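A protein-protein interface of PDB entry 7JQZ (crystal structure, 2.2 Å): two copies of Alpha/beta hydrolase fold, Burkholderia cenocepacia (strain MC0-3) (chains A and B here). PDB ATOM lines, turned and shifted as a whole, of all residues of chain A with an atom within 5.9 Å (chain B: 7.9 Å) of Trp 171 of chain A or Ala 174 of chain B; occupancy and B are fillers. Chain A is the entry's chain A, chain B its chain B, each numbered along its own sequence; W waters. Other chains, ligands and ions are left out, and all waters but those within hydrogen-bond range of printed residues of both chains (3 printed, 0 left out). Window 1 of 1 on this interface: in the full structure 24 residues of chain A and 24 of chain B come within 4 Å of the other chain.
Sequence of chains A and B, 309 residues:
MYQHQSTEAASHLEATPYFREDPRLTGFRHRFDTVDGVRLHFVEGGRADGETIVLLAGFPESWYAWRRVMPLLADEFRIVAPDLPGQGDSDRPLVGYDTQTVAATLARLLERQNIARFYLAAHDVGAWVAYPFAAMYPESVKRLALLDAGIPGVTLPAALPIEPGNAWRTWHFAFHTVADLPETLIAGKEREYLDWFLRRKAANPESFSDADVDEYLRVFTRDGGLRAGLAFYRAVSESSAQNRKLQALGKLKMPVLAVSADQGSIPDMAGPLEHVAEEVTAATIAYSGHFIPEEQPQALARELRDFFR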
ATOM      1  N   PRO A 161     -10.865  20.577  -4.718  1.00  0.00           N
ATOM      2  CA  PRO A 161     -10.093  19.401  -5.140  1.00  0.00           C
ATOM      3  C   PRO A 161     -10.603  18.711  -6.397  1.00  0.00           C
ATOM      4  O   PRO A 161     -11.797  18.715  -6.727  1.00  0.00           O
ATOM      5  CB  PRO A 161     -10.191  18.460  -3.932  1.00  0.00           C
ATOM      6  CG  PRO A 161     -11.389  18.902  -3.188  1.00  0.00           C
ATOM      7  CD  PRO A 161     -11.441  20.396  -3.371  1.00  0.00           C
ATOM      8  N   ILE A 162      -9.656  18.078  -7.086  1.00  0.00           N
ATOM      9  CA  ILE A 162      -9.905  17.305  -8.289  1.00  0.00           C
ATOM     10  C   ILE A 162      -9.581  15.836  -8.091  1.00  0.00           C
ATOM     11  O   ILE A 162      -9.761  15.041  -9.014  1.00  0.00           O
ATOM     12  CB  ILE A 162      -9.111  17.872  -9.482  1.00  0.00           C
ATOM     13  CG1 ILE A 162      -7.603  17.830  -9.179  1.00  0.00           C
ATOM     14  CG2 ILE A 162      -9.597  19.287  -9.786  1.00  0.00           C
ATOM     15  CD1 ILE A 162      -6.711  18.047 -10.399  1.00  0.00           C
ATOM     16  N   ALA A 167     -13.254  14.818  -5.282  1.00  0.00           N
ATOM     17  CA  ALA A 167     -13.805  15.782  -6.226  1.00  0.00           C
ATOM     18  C   ALA A 167     -15.335  15.752  -6.264  1.00  0.00           C
ATOM     19  O   ALA A 167     -15.960  16.805  -6.404  1.00  0.00           O
ATOM     20  CB  ALA A 167     -13.203  15.556  -7.613  1.00  0.00           C
ATOM     21  N   TRP A 168     -15.960  14.586  -6.068  1.00  0.00           N
ATOM     22  CA  TRP A 168     -17.419  14.508  -6.158  1.00  0.00           C
ATOM     23  C   TRP A 168     -18.133  15.381  -5.130  1.00  0.00           C
ATOM     24  O   TRP A 168     -19.307  15.715  -5.319  1.00  0.00           O
ATOM     25  CB  TRP A 168     -17.891  13.063  -6.012  1.00  0.00           C
ATOM     26  CG  TRP A 168     -17.587  12.450  -4.673  1.00  0.00           C
ATOM     27  CD1 TRP A 168     -16.456  11.761  -4.316  1.00  0.00           C
ATOM     28  CD2 TRP A 168     -18.432  12.454  -3.523  1.00  0.00           C
ATOM     29  NE1 TRP A 168     -16.547  11.345  -3.012  1.00  0.00           N
ATOM     30  CE2 TRP A 168     -17.751  11.757  -2.500  1.00  0.00           C
ATOM     31  CE3 TRP A 168     -19.700  12.980  -3.259  1.00  0.00           C
ATOM     32  CZ2 TRP A 168     -18.291  11.582  -1.225  1.00  0.00           C
ATOM     33  CZ3 TRP A 168     -20.244  12.803  -1.999  1.00  0.00           C
ATOM     34  CH2 TRP A 168     -19.535  12.106  -0.992  1.00  0.00           C
ATOM     35  N   ARG A 169     -17.442  15.790  -4.068  1.00  0.00           N
ATOM     36  CA  ARG A 169     -18.065  16.614  -3.042  1.00  0.00           C
ATOM     37  C   ARG A 169     -18.339  18.032  -3.523  1.00  0.00           C
ATOM     38  O   ARG A 169     -19.220  18.720  -2.981  1.00  0.00           O
ATOM     39  CB  ARG A 169     -17.168  16.656  -1.817  1.00  0.00           C
ATOM     40  CG  ARG A 169     -17.084  15.300  -1.165  1.00  0.00           C
ATOM     41  CD  ARG A 169     -17.118  15.431   0.318  1.00  0.00           C
ATOM     42  NE  ARG A 169     -17.320  14.137   0.958  1.00  0.00           N
ATOM     43  CZ  ARG A 169     -16.351  13.251   1.126  1.00  0.00           C
ATOM     44  NH1 ARG A 169     -15.133  13.529   0.691  1.00  0.00           N
ATOM     45  NH2 ARG A 169     -16.598  12.090   1.712  1.00  0.00           N
ATOM     46  N   THR A 170     -17.556  18.513  -4.472  1.00  0.00           N
ATOM     47  CA  THR A 170     -17.562  19.928  -4.801  1.00  0.00           C
ATOM     48  C   THR A 170     -17.520  20.200  -6.293  1.00  0.00           C
ATOM     49  O   THR A 170     -17.383  21.366  -6.681  1.00  0.00           O
ATOM     50  CB  THR A 170     -16.367  20.604  -4.121  1.00  0.00           C
ATOM     51  OG1 THR A 170     -15.166  19.942  -4.531  1.00  0.00           O
ATOM     52  CG2 THR A 170     -16.487  20.524  -2.587  1.00  0.00           C
ATOM     53  N   TRP A 171     -17.581  19.166  -7.137  1.00  0.00           N
ATOM     54  CA  TRP A 171     -17.446  19.367  -8.573  1.00  0.00           C
ATOM     55  C   TRP A 171     -18.503  20.317  -9.115  1.00  0.00           C
ATOM     56  O   TRP A 171     -18.262  21.011 -10.110  1.00  0.00           O
ATOM     57  CB  TRP A 171     -17.553  18.025  -9.302  1.00  0.00           C
ATOM     58  CG  TRP A 171     -18.967  17.522  -9.428  1.00  0.00           C
ATOM     59  CD1 TRP A 171     -19.637  16.726  -8.538  1.00  0.00           C
ATOM     60  CD2 TRP A 171     -19.896  17.811 -10.483  1.00  0.00           C
ATOM     61  NE1 TRP A 171     -20.913  16.474  -8.986  1.00  0.00           N
ATOM     62  CE2 TRP A 171     -21.100  17.131 -10.178  1.00  0.00           C
ATOM     63  CE3 TRP A 171     -19.823  18.574 -11.655  1.00  0.00           C
ATOM     64  CZ2 TRP A 171     -22.230  17.202 -10.994  1.00  0.00           C
ATOM     65  CZ3 TRP A 171     -20.936  18.626 -12.494  1.00  0.00           C
ATOM     66  CH2 TRP A 171     -22.133  17.932 -12.154  1.00  0.00           C
ATOM     67  N   HIS A 172     -19.680  20.327  -8.492  1.00  0.00           N
ATOM     68  CA  HIS A 172     -20.834  21.055  -9.004  1.00  0.00           C
ATOM     69  C   HIS A 172     -20.657  22.565  -8.904  1.00  0.00           C
ATOM     70  O   HIS A 172     -21.310  23.303  -9.658  1.00  0.00           O
ATOM     71  CB  HIS A 172     -22.088  20.610  -8.230  1.00  0.00           C
ATOM     72  CG  HIS A 172     -22.030  20.928  -6.761  1.00  0.00           C
ATOM     73  ND1 HIS A 172     -21.196  20.258  -5.889  1.00  0.00           N
ATOM     74  CD2 HIS A 172     -22.693  21.846  -6.012  1.00  0.00           C
ATOM     75  CE1 HIS A 172     -21.343  20.754  -4.671  1.00  0.00           C
ATOM     76  NE2 HIS A 172     -22.242  21.724  -4.717  1.00  0.00           N
ATOM     77  N   PHE A 173     -19.811  23.026  -7.971  1.00  0.00           N
ATOM     78  CA  PHE A 173     -19.557  24.452  -7.779  1.00  0.00           C
ATOM     79  C   PHE A 173     -19.130  25.108  -9.087  1.00  0.00           C
ATOM     80  O   PHE A 173     -19.779  26.032  -9.585  1.00  0.00           O
ATOM     81  CB  PHE A 173     -18.459  24.653  -6.713  1.00  0.00           C
ATOM     82  CG  PHE A 173     -18.970  24.793  -5.300  1.00  0.00           C
ATOM     83  CD1 PHE A 173     -19.405  26.017  -4.824  1.00  0.00           C
ATOM     84  CD2 PHE A 173     -18.978  23.709  -4.436  1.00  0.00           C
ATOM     85  CE1 PHE A 173     -19.853  26.148  -3.510  1.00  0.00           C
ATOM     86  CE2 PHE A 173     -19.434  23.829  -3.119  1.00  0.00           C
ATOM     87  CZ  PHE A 173     -19.876  25.047  -2.661  1.00  0.00           C
ATOM     88  N   ALA A 174     -18.017  24.637  -9.647  1.00  0.00           N
ATOM     89  CA  ALA A 174     -17.507  25.201 -10.889  1.00  0.00           C
ATOM     90  C   ALA A 174     -18.473  24.964 -12.049  1.00  0.00           C
ATOM     91  O   ALA A 174     -18.675  25.854 -12.887  1.00  0.00           O
ATOM     92  CB  ALA A 174     -16.131  24.610 -11.192  1.00  0.00           C
ATOM     93  N   PHE A 175     -19.081  23.775 -12.112  1.00  0.00           N
ATOM     94  CA  PHE A 175     -20.029  23.467 -13.183  1.00  0.00           C
ATOM     95  C   PHE A 175     -21.127  24.508 -13.244  1.00  0.00           C
ATOM     96  O   PHE A 175     -21.454  25.034 -14.311  1.00  0.00           O
ATOM     97  CB  PHE A 175     -20.645  22.098 -12.938  1.00  0.00           C
ATOM     98  CG  PHE A 175     -21.700  21.687 -13.936  1.00  0.00           C
ATOM     99  CD1 PHE A 175     -21.491  21.834 -15.297  1.00  0.00           C
ATOM    100  CD2 PHE A 175     -22.865  21.061 -13.507  1.00  0.00           C
ATOM    101  CE1 PHE A 175     -22.447  21.411 -16.214  1.00  0.00           C
ATOM    102  CE2 PHE A 175     -23.811  20.609 -14.423  1.00  0.00           C
ATOM    103  CZ  PHE A 175     -23.598  20.776 -15.772  1.00  0.00           C
ATOM    104  N   HIS A 176     -21.690  24.829 -12.085  1.00  0.00           N
ATOM    105  CA  HIS A 176     -22.833  25.724 -12.045  1.00  0.00           C
ATOM    106  C   HIS A 176     -22.487  27.135 -12.534  1.00  0.00           C
ATOM    107  O   HIS A 176     -23.395  27.851 -12.971  1.00  0.00           O
ATOM    108  CB  HIS A 176     -23.412  25.734 -10.622  1.00  0.00           C
ATOM    109  CG  HIS A 176     -24.129  24.465 -10.250  1.00  0.00           C
ATOM    110  ND1 HIS A 176     -24.567  24.200  -8.969  1.00  0.00           N
ATOM    111  CD2 HIS A 176     -24.480  23.385 -10.992  1.00  0.00           C
ATOM    112  CE1 HIS A 176     -25.170  23.022  -8.940  1.00  0.00           C
ATOM    113  NE2 HIS A 176     -25.126  22.504 -10.153  1.00  0.00           N
ATOM    114  N   TYR A 193     -30.450  14.102 -11.809  1.00  0.00           N
ATOM    115  CA  TYR A 193     -29.523  15.069 -11.240  1.00  0.00           C
ATOM    116  C   TYR A 193     -29.797  15.268  -9.753  1.00  0.00           C
ATOM    117  O   TYR A 193     -28.881  15.210  -8.932  1.00  0.00           O
ATOM    118  CB  TYR A 193     -29.629  16.387 -12.012  1.00  0.00           C
ATOM    119  CG  TYR A 193     -28.475  17.303 -11.775  1.00  0.00           C
ATOM    120  CD1 TYR A 193     -27.184  16.939 -12.153  1.00  0.00           C
ATOM    121  CD2 TYR A 193     -28.670  18.559 -11.203  1.00  0.00           C
ATOM    122  CE1 TYR A 193     -26.097  17.797 -11.920  1.00  0.00           C
ATOM    123  CE2 TYR A 193     -27.590  19.436 -10.975  1.00  0.00           C
ATOM    124  CZ  TYR A 193     -26.311  19.048 -11.343  1.00  0.00           C
ATOM    125  OH  TYR A 193     -25.259  19.903 -11.111  1.00  0.00           O
ATOM    126  N   TRP A 196     -28.957  12.142  -7.605  1.00  0.00           N
ATOM    127  CA  TRP A 196     -27.530  12.027  -7.343  1.00  0.00           C
ATOM    128  C   TRP A 196     -27.125  12.903  -6.163  1.00  0.00           C
ATOM    129  O   TRP A 196     -26.414  12.457  -5.262  1.00  0.00           O
ATOM    130  CB  TRP A 196     -26.729  12.401  -8.587  1.00  0.00           C
ATOM    131  CG  TRP A 196     -25.287  12.099  -8.397  1.00  0.00           C
ATOM    132  CD1 TRP A 196     -24.653  10.939  -8.723  1.00  0.00           C
ATOM    133  CD2 TRP A 196     -24.305  12.941  -7.788  1.00  0.00           C
ATOM    134  NE1 TRP A 196     -23.336  11.008  -8.378  1.00  0.00           N
ATOM    135  CE2 TRP A 196     -23.087  12.228  -7.805  1.00  0.00           C
ATOM    136  CE3 TRP A 196     -24.321  14.250  -7.272  1.00  0.00           C
ATOM    137  CZ2 TRP A 196     -21.891  12.763  -7.300  1.00  0.00           C
ATOM    138  CZ3 TRP A 196     -23.148  14.783  -6.767  1.00  0.00           C
ATOM    139  CH2 TRP A 196     -21.933  14.039  -6.790  1.00  0.00           C
ATOM    140  N   PHE A 197     -27.569  14.158  -6.148  1.00  0.00           N
ATOM    141  CA  PHE A 197     -27.155  15.053  -5.068  1.00  0.00           C
ATOM    142  C   PHE A 197     -27.591  14.526  -3.709  1.00  0.00           C
ATOM    143  O   PHE A 197     -26.782  14.409  -2.781  1.00  0.00           O
ATOM    144  CB  PHE A 197     -27.714  16.446  -5.322  1.00  0.00           C
ATOM    145  CG  PHE A 197     -26.787  17.285  -6.108  1.00  0.00           C
ATOM    146  CD1 PHE A 197     -26.855  17.299  -7.474  1.00  0.00           C
ATOM    147  CD2 PHE A 197     -25.793  17.991  -5.475  1.00  0.00           C
ATOM    148  CE1 PHE A 197     -25.951  18.042  -8.201  1.00  0.00           C
ATOM    149  CE2 PHE A 197     -24.901  18.728  -6.192  1.00  0.00           C
ATOM    150  CZ  PHE A 197     -24.985  18.758  -7.554  1.00  0.00           C
ATOM    151  N   LEU B 160      -8.344  23.031  -8.036  1.00  0.00           N
ATOM    152  CA  LEU B 160      -8.369  23.940  -9.180  1.00  0.00           C
ATOM    153  C   LEU B 160      -9.363  25.087  -8.968  1.00  0.00           C
ATOM    154  O   LEU B 160     -10.363  24.920  -8.263  1.00  0.00           O
ATOM    155  CB  LEU B 160      -8.728  23.180 -10.468  1.00  0.00           C
ATOM    156  CG  LEU B 160      -7.772  22.074 -10.934  1.00  0.00           C
ATOM    157  CD1 LEU B 160      -8.277  21.447 -12.237  1.00  0.00           C
ATOM    158  CD2 LEU B 160      -6.335  22.582 -11.087  1.00  0.00           C
ATOM    159  N   ILE B 162     -12.222  28.075  -8.867  1.00  0.00           N
ATOM    160  CA  ILE B 162     -13.658  28.024  -9.127  1.00  0.00           C
ATOM    161  C   ILE B 162     -14.305  29.367  -9.468  1.00  0.00           C
ATOM    162  O   ILE B 162     -15.465  29.406  -9.878  1.00  0.00           O
ATOM    163  CB  ILE B 162     -14.419  27.398  -7.941  1.00  0.00           C
ATOM    164  CG1 ILE B 162     -14.216  28.233  -6.675  1.00  0.00           C
ATOM    165  CG2 ILE B 162     -13.966  25.963  -7.714  1.00  0.00           C
ATOM    166  CD1 ILE B 162     -15.096  27.813  -5.519  1.00  0.00           C
ATOM    167  N   THR B 170     -11.686  24.593 -16.171  1.00  0.00           N
ATOM    168  CA  THR B 170     -11.246  23.391 -15.483  1.00  0.00           C
ATOM    169  C   THR B 170     -12.371  22.650 -14.763  1.00  0.00           C
ATOM    170  O   THR B 170     -12.092  21.648 -14.093  1.00  0.00           O
ATOM    171  CB  THR B 170     -10.136  23.744 -14.483  1.00  0.00           C
ATOM    172  OG1 THR B 170     -10.593  24.801 -13.635  1.00  0.00           O
ATOM    173  CG2 THR B 170      -8.850  24.185 -15.214  1.00  0.00           C
ATOM    174  N   TRP B 171     -13.629  23.101 -14.881  1.00  0.00           N
ATOM    175  CA  TRP B 171     -14.718  22.450 -14.148  1.00  0.00           C
ATOM    176  C   TRP B 171     -14.825  20.976 -14.513  1.00  0.00           C
ATOM    177  O   TRP B 171     -15.259  20.168 -13.689  1.00  0.00           O
ATOM    178  CB  TRP B 171     -16.056  23.140 -14.431  1.00  0.00           C
ATOM    179  CG  TRP B 171     -16.564  22.750 -15.763  1.00  0.00           C
ATOM    180  CD1 TRP B 171     -16.255  23.345 -16.953  1.00  0.00           C
ATOM    181  CD2 TRP B 171     -17.431  21.649 -16.077  1.00  0.00           C
ATOM    182  NE1 TRP B 171     -16.875  22.696 -17.976  1.00  0.00           N
ATOM    183  CE2 TRP B 171     -17.611  21.654 -17.471  1.00  0.00           C
ATOM    184  CE3 TRP B 171     -18.077  20.673 -15.318  1.00  0.00           C
ATOM    185  CZ2 TRP B 171     -18.414  20.725 -18.128  1.00  0.00           C
ATOM    186  CZ3 TRP B 171     -18.890  19.732 -15.989  1.00  0.00           C
ATOM    187  CH2 TRP B 171     -19.034  19.766 -17.369  1.00  0.00           C
ATOM    188  N   HIS B 172     -14.446  20.619 -15.737  1.00  0.00           N
ATOM    189  CA  HIS B 172     -14.650  19.259 -16.232  1.00  0.00           C
ATOM    190  C   HIS B 172     -13.778  18.220 -15.521  1.00  0.00           C
ATOM    191  O   HIS B 172     -14.166  17.041 -15.459  1.00  0.00           O
ATOM    192  CB  HIS B 172     -14.359  19.201 -17.726  1.00  0.00           C
ATOM    193  CG  HIS B 172     -12.925  19.490 -18.074  1.00  0.00           C
ATOM    194  ND1 HIS B 172     -12.384  20.759 -18.020  1.00  0.00           N
ATOM    195  CD2 HIS B 172     -11.923  18.674 -18.483  1.00  0.00           C
ATOM    196  CE1 HIS B 172     -11.113  20.714 -18.376  1.00  0.00           C
ATOM    197  NE2 HIS B 172     -10.805  19.459 -18.654  1.00  0.00           N
ATOM    198  N   PHE B 173     -12.605  18.630 -15.015  1.00  0.00           N
ATOM    199  CA  PHE B 173     -11.692  17.719 -14.329  1.00  0.00           C
ATOM    200  C   PHE B 173     -12.415  16.943 -13.237  1.00  0.00           C
ATOM    201  O   PHE B 173     -12.467  15.710 -13.259  1.00  0.00           O
ATOM    202  CB  PHE B 173     -10.514  18.496 -13.719  1.00  0.00           C
ATOM    203  CG  PHE B 173      -9.370  18.733 -14.666  1.00  0.00           C
ATOM    204  CD1 PHE B 173      -8.425  17.754 -14.891  1.00  0.00           C
ATOM    205  CD2 PHE B 173      -9.223  19.957 -15.313  1.00  0.00           C
ATOM    206  CE1 PHE B 173      -7.360  17.986 -15.767  1.00  0.00           C
ATOM    207  CE2 PHE B 173      -8.159  20.194 -16.179  1.00  0.00           C
ATOM    208  CZ  PHE B 173      -7.237  19.205 -16.410  1.00  0.00           C
ATOM    209  N   ALA B 174     -12.985  17.666 -12.272  1.00  0.00           N
ATOM    210  CA  ALA B 174     -13.696  17.040 -11.167  1.00  0.00           C
ATOM    211  C   ALA B 174     -14.953  16.300 -11.640  1.00  0.00           C
ATOM    212  O   ALA B 174     -15.242  15.206 -11.149  1.00  0.00           O
ATOM    213  CB  ALA B 174     -14.031  18.108 -10.117  1.00  0.00           C
ATOM    214  N   PHE B 175     -15.713  16.881 -12.584  1.00  0.00           N
ATOM    215  CA  PHE B 175     -16.909  16.215 -13.126  1.00  0.00           C
ATOM    216  C   PHE B 175     -16.569  14.829 -13.650  1.00  0.00           C
ATOM    217  O   PHE B 175     -17.260  13.843 -13.360  1.00  0.00           O
ATOM    218  CB  PHE B 175     -17.519  17.072 -14.253  1.00  0.00           C
ATOM    219  CG  PHE B 175     -18.785  16.479 -14.946  1.00  0.00           C
ATOM    220  CD1 PHE B 175     -19.873  16.025 -14.213  1.00  0.00           C
ATOM    221  CD2 PHE B 175     -18.881  16.466 -16.336  1.00  0.00           C
ATOM    222  CE1 PHE B 175     -21.026  15.537 -14.862  1.00  0.00           C
ATOM    223  CE2 PHE B 175     -20.027  15.994 -16.999  1.00  0.00           C
ATOM    224  CZ  PHE B 175     -21.101  15.540 -16.268  1.00  0.00           C
ATOM    225  N   HIS B 176     -15.484  14.738 -14.425  1.00  0.00           N
ATOM    226  CA  HIS B 176     -15.150  13.478 -15.076  1.00  0.00           C
ATOM    227  C   HIS B 176     -14.804  12.374 -14.086  1.00  0.00           C
ATOM    228  O   HIS B 176     -14.996  11.190 -14.406  1.00  0.00           O
ATOM    229  CB  HIS B 176     -14.017  13.697 -16.076  1.00  0.00           C
ATOM    230  CG  HIS B 176     -14.452  14.459 -17.283  1.00  0.00           C
ATOM    231  ND1 HIS B 176     -13.575  14.890 -18.254  1.00  0.00           N
ATOM    232  CD2 HIS B 176     -15.683  14.895 -17.659  1.00  0.00           C
ATOM    233  CE1 HIS B 176     -14.258  15.520 -19.201  1.00  0.00           C
ATOM    234  NE2 HIS B 176     -15.539  15.539 -18.861  1.00  0.00           N
ATOM    235  N   THR B 177     -14.357  12.724 -12.877  1.00  0.00           N
ATOM    236  CA  THR B 177     -14.031  11.680 -11.912  1.00  0.00           C
ATOM    237  C   THR B 177     -15.278  11.035 -11.327  1.00  0.00           C
ATOM    238  O   THR B 177     -15.171   9.948 -10.756  1.00  0.00           O
ATOM    239  CB  THR B 177     -13.173  12.211 -10.749  1.00  0.00           C
ATOM    240  OG1 THR B 177     -13.978  13.046  -9.912  1.00  0.00           O
ATOM    241  CG2 THR B 177     -11.959  13.014 -11.239  1.00  0.00           C
ATOM    242  N   VAL B 178     -16.444  11.682 -11.438  1.00  0.00           N
ATOM    243  CA  VAL B 178     -17.660  11.147 -10.830  1.00  0.00           C
ATOM    244  C   VAL B 178     -18.146   9.945 -11.627  1.00  0.00           C
ATOM    245  O   VAL B 178     -18.329  10.022 -12.851  1.00  0.00           O
ATOM    246  CB  VAL B 178     -18.749  12.229 -10.758  1.00  0.00           C
ATOM    247  CG1 VAL B 178     -20.068  11.635 -10.217  1.00  0.00           C
ATOM    248  CG2 VAL B 178     -18.279  13.421  -9.892  1.00  0.00           C
ATOM    249  N   ALA B 179     -18.418   8.848 -10.933  1.00  0.00           N
ATOM    250  CA  ALA B 179     -18.904   7.651 -11.608  1.00  0.00           C
ATOM    251  C   ALA B 179     -20.318   7.880 -12.129  1.00  0.00           C
ATOM    252  O   ALA B 179     -21.142   8.488 -11.454  1.00  0.00           O
ATOM    253  CB  ALA B 179     -18.883   6.453 -10.652  1.00  0.00           C
ATOM    254  N   LEU B 181     -22.592   9.550 -13.320  1.00  0.00           N
ATOM    255  CA  LEU B 181     -23.336  10.774 -13.605  1.00  0.00           C
ATOM    256  C   LEU B 181     -22.941  11.405 -14.937  1.00  0.00           C
ATOM    257  O   LEU B 181     -23.844  11.894 -15.643  1.00  0.00           O
ATOM    258  CB  LEU B 181     -23.166  11.794 -12.471  1.00  0.00           C
ATOM    259  CG  LEU B 181     -24.036  13.055 -12.629  1.00  0.00           C
ATOM    260  CD1 LEU B 181     -25.489  12.716 -12.584  1.00  0.00           C
ATOM    261  CD2 LEU B 181     -23.750  14.088 -11.563  1.00  0.00           C
ATOM    262  N   PRO B 182     -21.655  11.459 -15.323  1.00  0.00           N
ATOM    263  CA  PRO B 182     -21.320  12.074 -16.618  1.00  0.00           C
ATOM    264  C   PRO B 182     -21.975  11.372 -17.787  1.00  0.00           C
ATOM    265  O   PRO B 182     -22.581  12.036 -18.634  1.00  0.00           O
ATOM    266  CB  PRO B 182     -19.787  11.981 -16.655  1.00  0.00           C
ATOM    267  CG  PRO B 182     -19.381  12.040 -15.210  1.00  0.00           C
ATOM    268  CD  PRO B 182     -20.436  11.202 -14.521  1.00  0.00           C
ATOM    269  N   LEU B 185     -25.615  12.413 -17.871  1.00  0.00           N
ATOM    270  CA  LEU B 185     -25.943  13.763 -18.320  1.00  0.00           C
ATOM    271  C   LEU B 185     -25.526  14.016 -19.766  1.00  0.00           C
ATOM    272  O   LEU B 185     -26.168  14.811 -20.456  1.00  0.00           O
ATOM    273  CB  LEU B 185     -25.304  14.804 -17.403  1.00  0.00           C
ATOM    274  CG  LEU B 185     -25.818  14.810 -15.963  1.00  0.00           C
ATOM    275  CD1 LEU B 185     -25.125  15.931 -15.189  1.00  0.00           C
ATOM    276  CD2 LEU B 185     -27.321  15.005 -15.917  1.00  0.00           C
ATOM    277  N   TYR B 233      -9.374  10.544 -16.690  1.00  0.00           N
ATOM    278  CA  TYR B 233      -9.578  11.386 -15.520  1.00  0.00           C
ATOM    279  C   TYR B 233      -9.844  10.541 -14.289  1.00  0.00           C
ATOM    280  O   TYR B 233      -9.398  10.883 -13.192  1.00  0.00           O
ATOM    281  CB  TYR B 233     -10.732  12.368 -15.775  1.00  0.00           C
ATOM    282  CG  TYR B 233     -10.471  13.292 -16.940  1.00  0.00           C
ATOM    283  CD1 TYR B 233      -9.931  14.568 -16.742  1.00  0.00           C
ATOM    284  CD2 TYR B 233     -10.755  12.895 -18.243  1.00  0.00           C
ATOM    285  CE1 TYR B 233      -9.674  15.430 -17.828  1.00  0.00           C
ATOM    286  CE2 TYR B 233     -10.501  13.751 -19.334  1.00  0.00           C
ATOM    287  CZ  TYR B 233      -9.959  15.007 -19.105  1.00  0.00           C
ATOM    288  OH  TYR B 233      -9.718  15.828 -20.169  1.00  0.00           O
ATOM    289  N   ARG B 234     -10.549   9.415 -14.454  1.00  0.00           N
ATOM    290  CA  ARG B 234     -10.883   8.570 -13.309  1.00  0.00           C
ATOM    291  C   ARG B 234      -9.668   7.842 -12.736  1.00  0.00           C
ATOM    292  O   ARG B 234      -9.678   7.479 -11.555  1.00  0.00           O
ATOM    293  CB  ARG B 234     -11.973   7.569 -13.711  1.00  0.00           C
ATOM    294  CG  ARG B 234     -13.339   8.261 -13.847  1.00  0.00           C
ATOM    295  CD  ARG B 234     -14.316   7.606 -14.847  1.00  0.00           C
ATOM    296  NE  ARG B 234     -15.592   8.314 -14.757  1.00  0.00           N
ATOM    297  CZ  ARG B 234     -16.729   7.983 -15.373  1.00  0.00           C
ATOM    298  NH1 ARG B 234     -16.808   6.915 -16.150  1.00  0.00           N
ATOM    299  NH2 ARG B 234     -17.808   8.740 -15.198  1.00  0.00           N
HETATM  300  O   HOH W   1     -21.405   8.792  -8.741  1.00  0.00           O
HETATM  301  O   HOH W   2     -14.747  11.992  -7.566  1.00  0.00           O
HETATM  302  O   HOH W   3     -15.766  20.892 -11.213  1.00  0.00           O
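Of the printed residues of chain B, Ile 162 of chain A touches Leu 160 (3.5 Å) and Thr 177 (3.7 Å).
Of the printed residues of chain B, Ala 167 of chain A touches Ala 174 (3.7 Å) and Thr 177 (3.5 Å).
Trp 171 of chain A touches just these residues of chain B: Ala 174, Phe 175, Val 178 and Leu 181.
His 176 of chain A touches none of the printed residues of chain B.
Printed residues of chain B within 4 Å of Tyr 193 of chain A: Leu 185.
Thr 170 of chain B touches none of the printed residues of chain A.
Printed residues of chain A within 4 Å of Trp 171 of chain B: Ala 174 (3.6 Å) and Phe 175 (3.4 Å).
Printed residues of chain A within 4 Å of Ala 174 of chain B: Ala 167 (3.7 Å) and Trp 171 (3.6 Å).
Among the printed residues, merely in contact across the chains: Trp 171 of chain A with Phe 175 of chain B, Phe 175 of chain A with Trp 171 of chain B, Ala 167 of chain A with Thr 177 of chain B, Trp 171 of chain A with Leu 181 of chain B, Ile 162 of chain A with Leu 160 of chain B, Ala 174 of chain A with Trp 171 of chain B, Trp 171 of chain A with Ala 174 of chain B, Trp 196 of chain A with Val 178 of chain B, Ala 167 of chain A with Ala 174 of chain B, Ile 162 of chain A with Thr 177 of chain B, Tyr 193 of chain A with Leu 185 of chain B, Trp 171 of chain A with Val 178 of chain B, Trp 168 of chain A with Val 178 of chain B and Trp 196 of chain A with Leu 181 of chain B.
A ring nitrogen (NE2) of His 176 of chain A lies within hydrogen-bond range of the side-chain hydroxyl of Tyr 193 of chain A (2.8 Å).
O of Val 178 of chain B sits at hydrogen-bond distance from NH2 of Arg 234 of chain B.
The side-chain hydroxyl (OG1) of Thr 177 of chain B sits at hydrogen-bond distance from the backbone carbonyl oxygen (O) of Ala 174 of chain B (2.8 Å).
Water W3 bridges the backbone carbonyl oxygen (O) of Trp 171 of chain B (2.6 Å) and the backbone carbonyl oxygen (O) of Trp 171 of chain A (2.7 Å).
Water W2 lies within hydrogen-bond range of the side-chain hydroxyl of Thr 177 of chain B and the backbone NH of Trp 168 of chain A.
Water W1 lies within hydrogen-bond range of the backbone carbonyl oxygen (O) of Ala 179 of chain B (2.7 Å) and the indole nitrogen (NE1) of Trp 196 of chain A (3.0 Å).
Hydrophobic or aromatic side chains of chain B that line the printed part of chain A: Leu 160, Trp 171, Ala 174, Phe 175, Val 178, Leu 181 and Leu 185.
Among the printed residues, 14 pairs touch across the chains.
Trp 171 of chain A touches Ala 174 of chain B, and with the chains exchanged Ala 174 of chain A touches Trp 171 of chain B.
Trp 171 of chain A touches Phe 175 of chain B, and with the chains exchanged Phe 175 of chain A touches Trp 171 of chain B.
8 positions are printed for both chains.
Of the 14 pairs that touch across the chains among the printed residues, 4 have their exchanged pair printed and touching as well.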
